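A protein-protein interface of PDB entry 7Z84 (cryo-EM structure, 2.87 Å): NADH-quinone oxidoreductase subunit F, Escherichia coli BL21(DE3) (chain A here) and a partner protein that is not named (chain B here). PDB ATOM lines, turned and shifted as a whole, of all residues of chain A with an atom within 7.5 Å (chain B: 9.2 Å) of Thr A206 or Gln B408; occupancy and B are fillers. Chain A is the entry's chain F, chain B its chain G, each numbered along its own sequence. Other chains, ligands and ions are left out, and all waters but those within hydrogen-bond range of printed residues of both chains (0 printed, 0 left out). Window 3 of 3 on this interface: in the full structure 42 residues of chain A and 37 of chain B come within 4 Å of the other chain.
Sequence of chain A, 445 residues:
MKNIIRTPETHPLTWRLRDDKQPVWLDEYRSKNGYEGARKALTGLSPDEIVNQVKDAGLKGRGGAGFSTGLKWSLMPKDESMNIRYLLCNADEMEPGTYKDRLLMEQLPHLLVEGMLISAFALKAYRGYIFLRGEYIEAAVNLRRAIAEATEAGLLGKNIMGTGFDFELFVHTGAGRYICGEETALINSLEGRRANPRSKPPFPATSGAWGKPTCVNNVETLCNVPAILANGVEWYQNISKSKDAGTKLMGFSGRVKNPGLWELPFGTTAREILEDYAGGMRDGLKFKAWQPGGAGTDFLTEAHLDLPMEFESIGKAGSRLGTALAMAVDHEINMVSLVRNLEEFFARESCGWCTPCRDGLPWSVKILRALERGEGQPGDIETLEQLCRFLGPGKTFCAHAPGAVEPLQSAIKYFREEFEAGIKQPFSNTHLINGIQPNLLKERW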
ATOM      1  N   LEU A  75      -9.819 -22.935   8.859  1.00  0.00           N
ATOM      2  CA  LEU A  75     -11.026 -22.739   9.650  1.00  0.00           C
ATOM      3  C   LEU A  75     -11.454 -23.991  10.401  1.00  0.00           C
ATOM      4  O   LEU A  75     -12.546 -24.006  10.977  1.00  0.00           O
ATOM      5  CB  LEU A  75     -12.178 -22.247   8.769  1.00  0.00           C
ATOM      6  CG  LEU A  75     -11.914 -20.954   7.999  1.00  0.00           C
ATOM      7  CD1 LEU A  75     -13.116 -20.574   7.160  1.00  0.00           C
ATOM      8  CD2 LEU A  75     -11.543 -19.829   8.951  1.00  0.00           C
ATOM      9  N   MET A  76     -10.635 -25.036  10.389  1.00  0.00           N
ATOM     10  CA  MET A  76     -10.863 -26.170  11.263  1.00  0.00           C
ATOM     11  C   MET A  76     -10.673 -25.735  12.717  1.00  0.00           C
ATOM     12  O   MET A  76      -9.857 -24.855  13.003  1.00  0.00           O
ATOM     13  CB  MET A  76      -9.899 -27.302  10.921  1.00  0.00           C
ATOM     14  CG  MET A  76     -10.373 -28.195   9.788  1.00  0.00           C
ATOM     15  SD  MET A  76     -11.631 -29.380  10.282  1.00  0.00           S
ATOM     16  CE  MET A  76     -11.131 -30.819   9.340  1.00  0.00           C
ATOM     17  N   PRO A  77     -11.440 -26.308  13.647  1.00  0.00           N
ATOM     18  CA  PRO A  77     -11.353 -25.870  15.045  1.00  0.00           C
ATOM     19  C   PRO A  77     -10.001 -26.183  15.666  1.00  0.00           C
ATOM     20  O   PRO A  77      -9.353 -27.180  15.342  1.00  0.00           O
ATOM     21  CB  PRO A  77     -12.474 -26.660  15.736  1.00  0.00           C
ATOM     22  CG  PRO A  77     -13.391 -27.068  14.634  1.00  0.00           C
ATOM     23  CD  PRO A  77     -12.510 -27.299  13.453  1.00  0.00           C
ATOM     24  N   ASP A  79      -9.568 -26.636  18.949  1.00  0.00           N
ATOM     25  CA  ASP A  79      -9.716 -27.380  20.192  1.00  0.00           C
ATOM     26  C   ASP A  79      -9.111 -28.770  20.052  1.00  0.00           C
ATOM     27  O   ASP A  79      -9.392 -29.488  19.088  1.00  0.00           O
ATOM     28  CB  ASP A  79     -11.192 -27.484  20.577  1.00  0.00           C
ATOM     29  CG  ASP A  79     -11.966 -26.219  20.272  1.00  0.00           C
ATOM     30  OD1 ASP A  79     -11.387 -25.120  20.406  1.00  0.00           O
ATOM     31  OD2 ASP A  79     -13.154 -26.322  19.900  1.00  0.00           O
ATOM     32  N   MET A  82     -11.620 -32.059  20.069  1.00  0.00           N
ATOM     33  CA  MET A  82     -12.235 -32.598  18.857  1.00  0.00           C
ATOM     34  C   MET A  82     -11.189 -33.382  18.062  1.00  0.00           C
ATOM     35  O   MET A  82     -10.672 -32.944  17.033  1.00  0.00           O
ATOM     36  CB  MET A  82     -12.852 -31.479  18.029  1.00  0.00           C
ATOM     37  CG  MET A  82     -13.841 -30.614  18.788  1.00  0.00           C
ATOM     38  SD  MET A  82     -14.320 -29.140  17.865  1.00  0.00           S
ATOM     39  CE  MET A  82     -15.625 -28.495  18.906  1.00  0.00           C
ATOM     40  N   PRO A 202     -23.707 -23.266  10.131  1.00  0.00           N
ATOM     41  CA  PRO A 202     -22.305 -23.687  10.246  1.00  0.00           C
ATOM     42  C   PRO A 202     -21.760 -24.408   9.016  1.00  0.00           C
ATOM     43  O   PRO A 202     -22.452 -25.201   8.382  1.00  0.00           O
ATOM     44  CB  PRO A 202     -22.326 -24.629  11.450  1.00  0.00           C
ATOM     45  CG  PRO A 202     -23.679 -25.206  11.434  1.00  0.00           C
ATOM     46  CD  PRO A 202     -24.597 -24.132  10.921  1.00  0.00           C
ATOM     47  N   PHE A 203     -20.513 -24.104   8.691  1.00  0.00           N
ATOM     48  CA  PHE A 203     -19.814 -24.748   7.598  1.00  0.00           C
ATOM     49  C   PHE A 203     -19.338 -26.129   8.035  1.00  0.00           C
ATOM     50  O   PHE A 203     -19.244 -26.405   9.234  1.00  0.00           O
ATOM     51  CB  PHE A 203     -18.653 -23.864   7.150  1.00  0.00           C
ATOM     52  CG  PHE A 203     -19.097 -22.604   6.469  1.00  0.00           C
ATOM     53  CD1 PHE A 203     -19.359 -22.592   5.109  1.00  0.00           C
ATOM     54  CD2 PHE A 203     -19.285 -21.439   7.194  1.00  0.00           C
ATOM     55  CE1 PHE A 203     -19.782 -21.439   4.482  1.00  0.00           C
ATOM     56  CE2 PHE A 203     -19.710 -20.281   6.572  1.00  0.00           C
ATOM     57  CZ  PHE A 203     -19.959 -20.282   5.215  1.00  0.00           C
ATOM     58  N   PRO A 204     -19.071 -27.033   7.084  1.00  0.00           N
ATOM     59  CA  PRO A 204     -18.632 -28.389   7.460  1.00  0.00           C
ATOM     60  C   PRO A 204     -17.327 -28.442   8.234  1.00  0.00           C
ATOM     61  O   PRO A 204     -17.082 -29.443   8.919  1.00  0.00           O
ATOM     62  CB  PRO A 204     -18.502 -29.095   6.108  1.00  0.00           C
ATOM     63  CG  PRO A 204     -19.503 -28.421   5.258  1.00  0.00           C
ATOM     64  CD  PRO A 204     -19.465 -26.976   5.662  1.00  0.00           C
ATOM     65  N   ALA A 205     -16.483 -27.410   8.144  1.00  0.00           N
ATOM     66  CA  ALA A 205     -15.256 -27.379   8.935  1.00  0.00           C
ATOM     67  C   ALA A 205     -15.550 -27.337  10.428  1.00  0.00           C
ATOM     68  O   ALA A 205     -14.811 -27.926  11.222  1.00  0.00           O
ATOM     69  CB  ALA A 205     -14.400 -26.183   8.527  1.00  0.00           C
ATOM     70  N   THR A 206     -16.629 -26.665  10.827  1.00  0.00           N
ATOM     71  CA  THR A 206     -17.015 -26.591  12.230  1.00  0.00           C
ATOM     72  C   THR A 206     -17.815 -27.819  12.655  1.00  0.00           C
ATOM     73  O   THR A 206     -17.505 -28.444  13.675  1.00  0.00           O
ATOM     74  CB  THR A 206     -17.809 -25.300  12.477  1.00  0.00           C
ATOM     75  OG1 THR A 206     -16.898 -24.204  12.619  1.00  0.00           O
ATOM     76  CG2 THR A 206     -18.657 -25.398  13.739  1.00  0.00           C
ATOM     77  N   SER A 207     -18.830 -28.194  11.874  1.00  0.00           N
ATOM     78  CA  SER A 207     -19.660 -29.355  12.195  1.00  0.00           C
ATOM     79  C   SER A 207     -20.131 -29.961  10.876  1.00  0.00           C
ATOM     80  O   SER A 207     -21.097 -29.477  10.278  1.00  0.00           O
ATOM     81  CB  SER A 207     -20.833 -28.962  13.083  1.00  0.00           C
ATOM     82  OG  SER A 207     -21.751 -28.144  12.382  1.00  0.00           O
ATOM     83  N   GLY A 208     -19.446 -31.012  10.434  1.00  0.00           N
ATOM     84  CA  GLY A 208     -19.744 -31.625   9.156  1.00  0.00           C
ATOM     85  C   GLY A 208     -20.314 -33.024   9.247  1.00  0.00           C
ATOM     86  O   GLY A 208     -21.498 -33.202   9.545  1.00  0.00           O
ATOM     87  N   ALA A 209     -19.477 -34.025   8.991  1.00  0.00           N
ATOM     88  CA  ALA A 209     -19.927 -35.410   8.946  1.00  0.00           C
ATOM     89  C   ALA A 209     -20.140 -35.931  10.360  1.00  0.00           C
ATOM     90  O   ALA A 209     -19.197 -35.971  11.158  1.00  0.00           O
ATOM     91  CB  ALA A 209     -18.915 -36.273   8.196  1.00  0.00           C
ATOM     92  N   GLY A 211     -21.612 -34.530  12.782  1.00  0.00           N
ATOM     93  CA  GLY A 211     -21.361 -33.488  13.751  1.00  0.00           C
ATOM     94  C   GLY A 211     -19.903 -33.178  14.000  1.00  0.00           C
ATOM     95  O   GLY A 211     -19.606 -32.218  14.721  1.00  0.00           O
ATOM     96  N   LYS A 212     -18.990 -33.950  13.436  1.00  0.00           N
ATOM     97  CA  LYS A 212     -17.562 -33.791  13.642  1.00  0.00           C
ATOM     98  C   LYS A 212     -16.982 -32.826  12.621  1.00  0.00           C
ATOM     99  O   LYS A 212     -17.588 -32.577  11.576  1.00  0.00           O
ATOM    100  CB  LYS A 212     -16.871 -35.148  13.539  1.00  0.00           C
ATOM    101  CG  LYS A 212     -17.553 -36.236  14.346  1.00  0.00           C
ATOM    102  CD  LYS A 212     -17.519 -35.919  15.829  1.00  0.00           C
ATOM    103  CE  LYS A 212     -18.074 -37.065  16.651  1.00  0.00           C
ATOM    104  NZ  LYS A 212     -19.523 -37.276  16.391  1.00  0.00           N
ATOM    105  N   PRO A 213     -15.830 -32.225  12.922  1.00  0.00           N
ATOM    106  CA  PRO A 213     -15.143 -31.400  11.919  1.00  0.00           C
ATOM    107  C   PRO A 213     -14.769 -32.202  10.677  1.00  0.00           C
ATOM    108  O   PRO A 213     -14.181 -33.287  10.755  1.00  0.00           O
ATOM    109  CB  PRO A 213     -13.904 -30.887  12.665  1.00  0.00           C
ATOM    110  CG  PRO A 213     -13.994 -31.428  14.066  1.00  0.00           C
ATOM    111  CD  PRO A 213     -15.374 -31.915  14.284  1.00  0.00           C
ATOM    112  N   THR A 214     -15.118 -31.643   9.521  1.00  0.00           N
ATOM    113  CA  THR A 214     -15.041 -32.330   8.244  1.00  0.00           C
ATOM    114  C   THR A 214     -14.553 -31.357   7.183  1.00  0.00           C
ATOM    115  O   THR A 214     -14.982 -30.202   7.149  1.00  0.00           O
ATOM    116  CB  THR A 214     -16.414 -32.896   7.853  1.00  0.00           C
ATOM    117  OG1 THR A 214     -16.915 -33.707   8.922  1.00  0.00           O
ATOM    118  CG2 THR A 214     -16.320 -33.741   6.608  1.00  0.00           C
ATOM    119  N   CYS A 215     -13.652 -31.816   6.324  1.00  0.00           N
ATOM    120  CA  CYS A 215     -13.192 -31.021   5.193  1.00  0.00           C
ATOM    121  C   CYS A 215     -13.435 -31.784   3.901  1.00  0.00           C
ATOM    122  O   CYS A 215     -12.981 -32.921   3.756  1.00  0.00           O
ATOM    123  CB  CYS A 215     -11.713 -30.669   5.322  1.00  0.00           C
ATOM    124  SG  CYS A 215     -11.138 -29.553   4.031  1.00  0.00           S
ATOM    125  N   ALA B 401     -28.931 -32.299  22.912  1.00  0.00           N
ATOM    126  CA  ALA B 401     -28.487 -31.828  21.605  1.00  0.00           C
ATOM    127  C   ALA B 401     -28.661 -30.323  21.486  1.00  0.00           C
ATOM    128  O   ALA B 401     -27.826 -29.637  20.877  1.00  0.00           O
ATOM    129  CB  ALA B 401     -29.253 -32.548  20.496  1.00  0.00           C
ATOM    130  N   ARG B 402     -29.732 -29.789  22.089  1.00  0.00           N
ATOM    131  CA  ARG B 402     -29.938 -28.341  22.106  1.00  0.00           C
ATOM    132  C   ARG B 402     -28.785 -27.614  22.795  1.00  0.00           C
ATOM    133  O   ARG B 402     -28.243 -26.640  22.262  1.00  0.00           O
ATOM    134  CB  ARG B 402     -31.262 -28.005  22.790  1.00  0.00           C
ATOM    135  CG  ARG B 402     -32.471 -28.125  21.891  1.00  0.00           C
ATOM    136  CD  ARG B 402     -33.666 -27.416  22.491  1.00  0.00           C
ATOM    137  NE  ARG B 402     -34.186 -28.104  23.667  1.00  0.00           N
ATOM    138  CZ  ARG B 402     -35.077 -29.085  23.627  1.00  0.00           C
ATOM    139  NH1 ARG B 402     -35.546 -29.545  22.478  1.00  0.00           N
ATOM    140  NH2 ARG B 402     -35.509 -29.616  24.766  1.00  0.00           N
ATOM    141  N   GLU B 403     -28.373 -28.090  23.973  1.00  0.00           N
ATOM    142  CA  GLU B 403     -27.297 -27.408  24.690  1.00  0.00           C
ATOM    143  C   GLU B 403     -25.927 -27.675  24.072  1.00  0.00           C
ATOM    144  O   GLU B 403     -25.036 -26.821  24.169  1.00  0.00           O
ATOM    145  CB  GLU B 403     -27.304 -27.791  26.174  1.00  0.00           C
ATOM    146  CG  GLU B 403     -26.909 -29.220  26.486  1.00  0.00           C
ATOM    147  CD  GLU B 403     -26.143 -29.339  27.785  1.00  0.00           C
ATOM    148  OE1 GLU B 403     -26.379 -28.515  28.692  1.00  0.00           O
ATOM    149  OE2 GLU B 403     -25.302 -30.255  27.898  1.00  0.00           O
ATOM    150  N   MET B 404     -25.738 -28.836  23.431  1.00  0.00           N
ATOM    151  CA  MET B 404     -24.501 -29.086  22.698  1.00  0.00           C
ATOM    152  C   MET B 404     -24.357 -28.125  21.527  1.00  0.00           C
ATOM    153  O   MET B 404     -23.261 -27.620  21.260  1.00  0.00           O
ATOM    154  CB  MET B 404     -24.456 -30.529  22.201  1.00  0.00           C
ATOM    155  CG  MET B 404     -23.936 -31.533  23.210  1.00  0.00           C
ATOM    156  SD  MET B 404     -24.151 -33.224  22.633  1.00  0.00           S
ATOM    157  CE  MET B 404     -23.046 -33.232  21.226  1.00  0.00           C
ATOM    158  N   ALA B 405     -25.454 -27.866  20.810  1.00  0.00           N
ATOM    159  CA  ALA B 405     -25.404 -26.878  19.741  1.00  0.00           C
ATOM    160  C   ALA B 405     -25.271 -25.464  20.290  1.00  0.00           C
ATOM    161  O   ALA B 405     -24.653 -24.609  19.646  1.00  0.00           O
ATOM    162  CB  ALA B 405     -26.643 -26.989  18.863  1.00  0.00           C
ATOM    163  N   ALA B 406     -25.850 -25.197  21.464  1.00  0.00           N
ATOM    164  CA  ALA B 406     -25.687 -23.892  22.097  1.00  0.00           C
ATOM    165  C   ALA B 406     -24.242 -23.641  22.509  1.00  0.00           C
ATOM    166  O   ALA B 406     -23.797 -22.489  22.526  1.00  0.00           O
ATOM    167  CB  ALA B 406     -26.609 -23.775  23.309  1.00  0.00           C
ATOM    168  N   ALA B 407     -23.498 -24.699  22.842  1.00  0.00           N
ATOM    169  CA  ALA B 407     -22.092 -24.539  23.198  1.00  0.00           C
ATOM    170  C   ALA B 407     -21.216 -24.175  22.003  1.00  0.00           C
ATOM    171  O   ALA B 407     -20.087 -23.715  22.201  1.00  0.00           O
ATOM    172  CB  ALA B 407     -21.566 -25.816  23.852  1.00  0.00           C
ATOM    173  N   GLN B 408     -21.702 -24.366  20.776  1.00  0.00           N
ATOM    174  CA  GLN B 408     -20.954 -24.040  19.570  1.00  0.00           C
ATOM    175  C   GLN B 408     -21.445 -22.759  18.905  1.00  0.00           C
ATOM    176  O   GLN B 408     -21.190 -22.559  17.711  1.00  0.00           O
ATOM    177  CB  GLN B 408     -21.012 -25.201  18.579  1.00  0.00           C
ATOM    178  CG  GLN B 408     -20.350 -26.474  19.068  1.00  0.00           C
ATOM    179  CD  GLN B 408     -19.992 -27.410  17.933  1.00  0.00           C
ATOM    180  OE1 GLN B 408     -19.867 -26.990  16.783  1.00  0.00           O
ATOM    181  NE2 GLN B 408     -19.824 -28.688  18.250  1.00  0.00           N
ATOM    182  N   LYS B 409     -22.145 -21.900  19.656  1.00  0.00           N
ATOM    183  CA  LYS B 409     -22.661 -20.609  19.182  1.00  0.00           C
ATOM    184  C   LYS B 409     -23.601 -20.771  17.988  1.00  0.00           C
ATOM    185  O   LYS B 409     -23.588 -19.973  17.049  1.00  0.00           O
ATOM    186  CB  LYS B 409     -21.526 -19.631  18.853  1.00  0.00           C
ATOM    187  CG  LYS B 409     -20.606 -19.291  20.022  1.00  0.00           C
ATOM    188  CD  LYS B 409     -21.368 -19.112  21.327  1.00  0.00           C
ATOM    189  CE  LYS B 409     -20.597 -19.697  22.499  1.00  0.00           C
ATOM    190  NZ  LYS B 409     -21.456 -19.866  23.704  1.00  0.00           N
ATOM    191  N   VAL B 410     -24.425 -21.814  18.025  1.00  0.00           N
ATOM    192  CA  VAL B 410     -25.454 -22.048  17.021  1.00  0.00           C
ATOM    193  C   VAL B 410     -26.787 -21.613  17.611  1.00  0.00           C
ATOM    194  O   VAL B 410     -27.103 -21.948  18.760  1.00  0.00           O
ATOM    195  CB  VAL B 410     -25.486 -23.524  16.585  1.00  0.00           C
ATOM    196  CG1 VAL B 410     -26.626 -23.784  15.617  1.00  0.00           C
ATOM    197  CG2 VAL B 410     -24.161 -23.916  15.957  1.00  0.00           C
ATOM    198  N   ALA B 411     -27.557 -20.849  16.838  1.00  0.00           N
ATOM    199  CA  ALA B 411     -28.825 -20.313  17.313  1.00  0.00           C
ATOM    200  C   ALA B 411     -29.842 -21.425  17.550  1.00  0.00           C
ATOM    201  O   ALA B 411     -29.826 -22.468  16.893  1.00  0.00           O
ATOM    202  CB  ALA B 411     -29.375 -19.300  16.314  1.00  0.00           C
ATOM    203  N   GLN B 414     -32.137 -22.686  14.581  1.00  0.00           N
ATOM    204  CA  GLN B 414     -31.519 -23.375  13.448  1.00  0.00           C
ATOM    205  C   GLN B 414     -31.477 -24.865  13.769  1.00  0.00           C
ATOM    206  O   GLN B 414     -30.445 -25.428  14.140  1.00  0.00           O
ATOM    207  CB  GLN B 414     -30.134 -22.811  13.170  1.00  0.00           C
ATOM    208  CG  GLN B 414     -29.737 -22.861  11.712  1.00  0.00           C
ATOM    209  CD  GLN B 414     -28.358 -22.295  11.465  1.00  0.00           C
ATOM    210  OE1 GLN B 414     -27.903 -21.402  12.180  1.00  0.00           O
ATOM    211  NE2 GLN B 414     -27.687 -22.804  10.442  1.00  0.00           N
ATOM    212  N   ALA B 417     -28.925 -27.652  12.170  1.00  0.00           N
ATOM    213  CA  ALA B 417     -27.579 -27.668  12.737  1.00  0.00           C
ATOM    214  C   ALA B 417     -27.577 -28.254  14.143  1.00  0.00           C
ATOM    215  O   ALA B 417     -26.614 -28.920  14.542  1.00  0.00           O
ATOM    216  CB  ALA B 417     -26.999 -26.258  12.746  1.00  0.00           C
ATOM    217  N   ILE B 418     -28.645 -28.005  14.907  1.00  0.00           N
ATOM    218  CA  ILE B 418     -28.767 -28.561  16.252  1.00  0.00           C
ATOM    219  C   ILE B 418     -28.836 -30.081  16.197  1.00  0.00           C
ATOM    220  O   ILE B 418     -28.160 -30.777  16.964  1.00  0.00           O
ATOM    221  CB  ILE B 418     -29.999 -27.965  16.959  1.00  0.00           C
ATOM    222  CG1 ILE B 418     -29.824 -26.460  17.162  1.00  0.00           C
ATOM    223  CG2 ILE B 418     -30.244 -28.648  18.293  1.00  0.00           C
ATOM    224  CD1 ILE B 418     -31.069 -25.766  17.637  1.00  0.00           C
ATOM    225  N   ASN B 420     -27.771 -31.905  13.710  1.00  0.00           N
ATOM    226  CA  ASN B 420     -26.522 -32.404  13.146  1.00  0.00           C
ATOM    227  C   ASN B 420     -25.425 -32.481  14.201  1.00  0.00           C
ATOM    228  O   ASN B 420     -24.628 -33.426  14.203  1.00  0.00           O
ATOM    229  CB  ASN B 420     -26.080 -31.520  11.982  1.00  0.00           C
ATOM    230  CG  ASN B 420     -24.742 -31.937  11.415  1.00  0.00           C
ATOM    231  OD1 ASN B 420     -24.576 -33.063  10.949  1.00  0.00           O
ATOM    232  ND2 ASN B 420     -23.775 -31.029  11.453  1.00  0.00           N
ATOM    233  N   ILE B 421     -25.358 -31.495  15.097  1.00  0.00           N
ATOM    234  CA  ILE B 421     -24.310 -31.490  16.116  1.00  0.00           C
ATOM    235  C   ILE B 421     -24.577 -32.571  17.158  1.00  0.00           C
ATOM    236  O   ILE B 421     -23.721 -33.422  17.427  1.00  0.00           O
ATOM    237  CB  ILE B 421     -24.197 -30.097  16.758  1.00  0.00           C
ATOM    238  CG1 ILE B 421     -23.542 -29.121  15.783  1.00  0.00           C
ATOM    239  CG2 ILE B 421     -23.399 -30.161  18.050  1.00  0.00           C
ATOM    240  CD1 ILE B 421     -23.681 -27.674  16.188  1.00  0.00           C
ATOM    241  N   GLY B 422     -25.762 -32.552  17.757  1.00  0.00           N
ATOM    242  CA  GLY B 422     -26.189 -33.600  18.660  1.00  0.00           C
ATOM    243  C   GLY B 422     -26.788 -34.775  17.918  1.00  0.00           C
ATOM    244  O   GLY B 422     -28.015 -34.907  17.860  1.00  0.00           O
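The side-chain amide oxygen (OD1) of Asn B420 lies close to the backbone carbonyl oxygen (O) of Gly A208 (3.4 Å).
The backbone carbonyl oxygen (O) of Ser A207 is in hydrogen-bond range of the side-chain amide nitrogen (ND2) of Asn B420.
Among the printed residues, merely in contact across the chains: Gly A211 with Asn B420 (3.3 Å), Pro A202 with Gln B414 (3.4 Å), Thr A206 with Gln B408 (3.6 Å), Pro A202 with Ala B417 (3.7 Å) and Ser A207 with Ile B421 (3.8 Å).
Thr A206 touches one residue of chain B.
Ser A207 touches two residues of chain B.
Arg B402 touches none of the printed residues of chain A.
No residue of chain A comes within 4 Å of Ala B407.
Gln B408 touches just one residue of chain A: Thr A206 (3.6 Å).
Printed residues of chain A within 4 Å of Gln B414: Pro A202.
Of the printed residues of chain A, Asn B420 touches Ser A207, Gly A208 and Gly A211.
Of the 18 printed residues of chain A, 5 touch a printed residue of chain B.
Printed residues of chain A that touch a printed residue of chain B: Pro A202, Thr A206, Ser A207, Gly A208 and Gly A211.
Hydrophobic or aromatic side chains of chain A that line the printed part of chain B: Pro A202.
Printed residues of chain B that touch a printed residue of chain A: Gln B408, Gln B414, Ala B417, Asn B420 and Ile B421.
Hydrophobic or aromatic side chains of chain B that line the printed part of chain A: Ala B417 and Ile B421.
Among the printed residues, 7 pairs touch across the chains.
Among the printed residues, no Asp or Glu carboxylate lies within 4 Å of a Lys or Arg side-chain nitrogen of the other chain.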
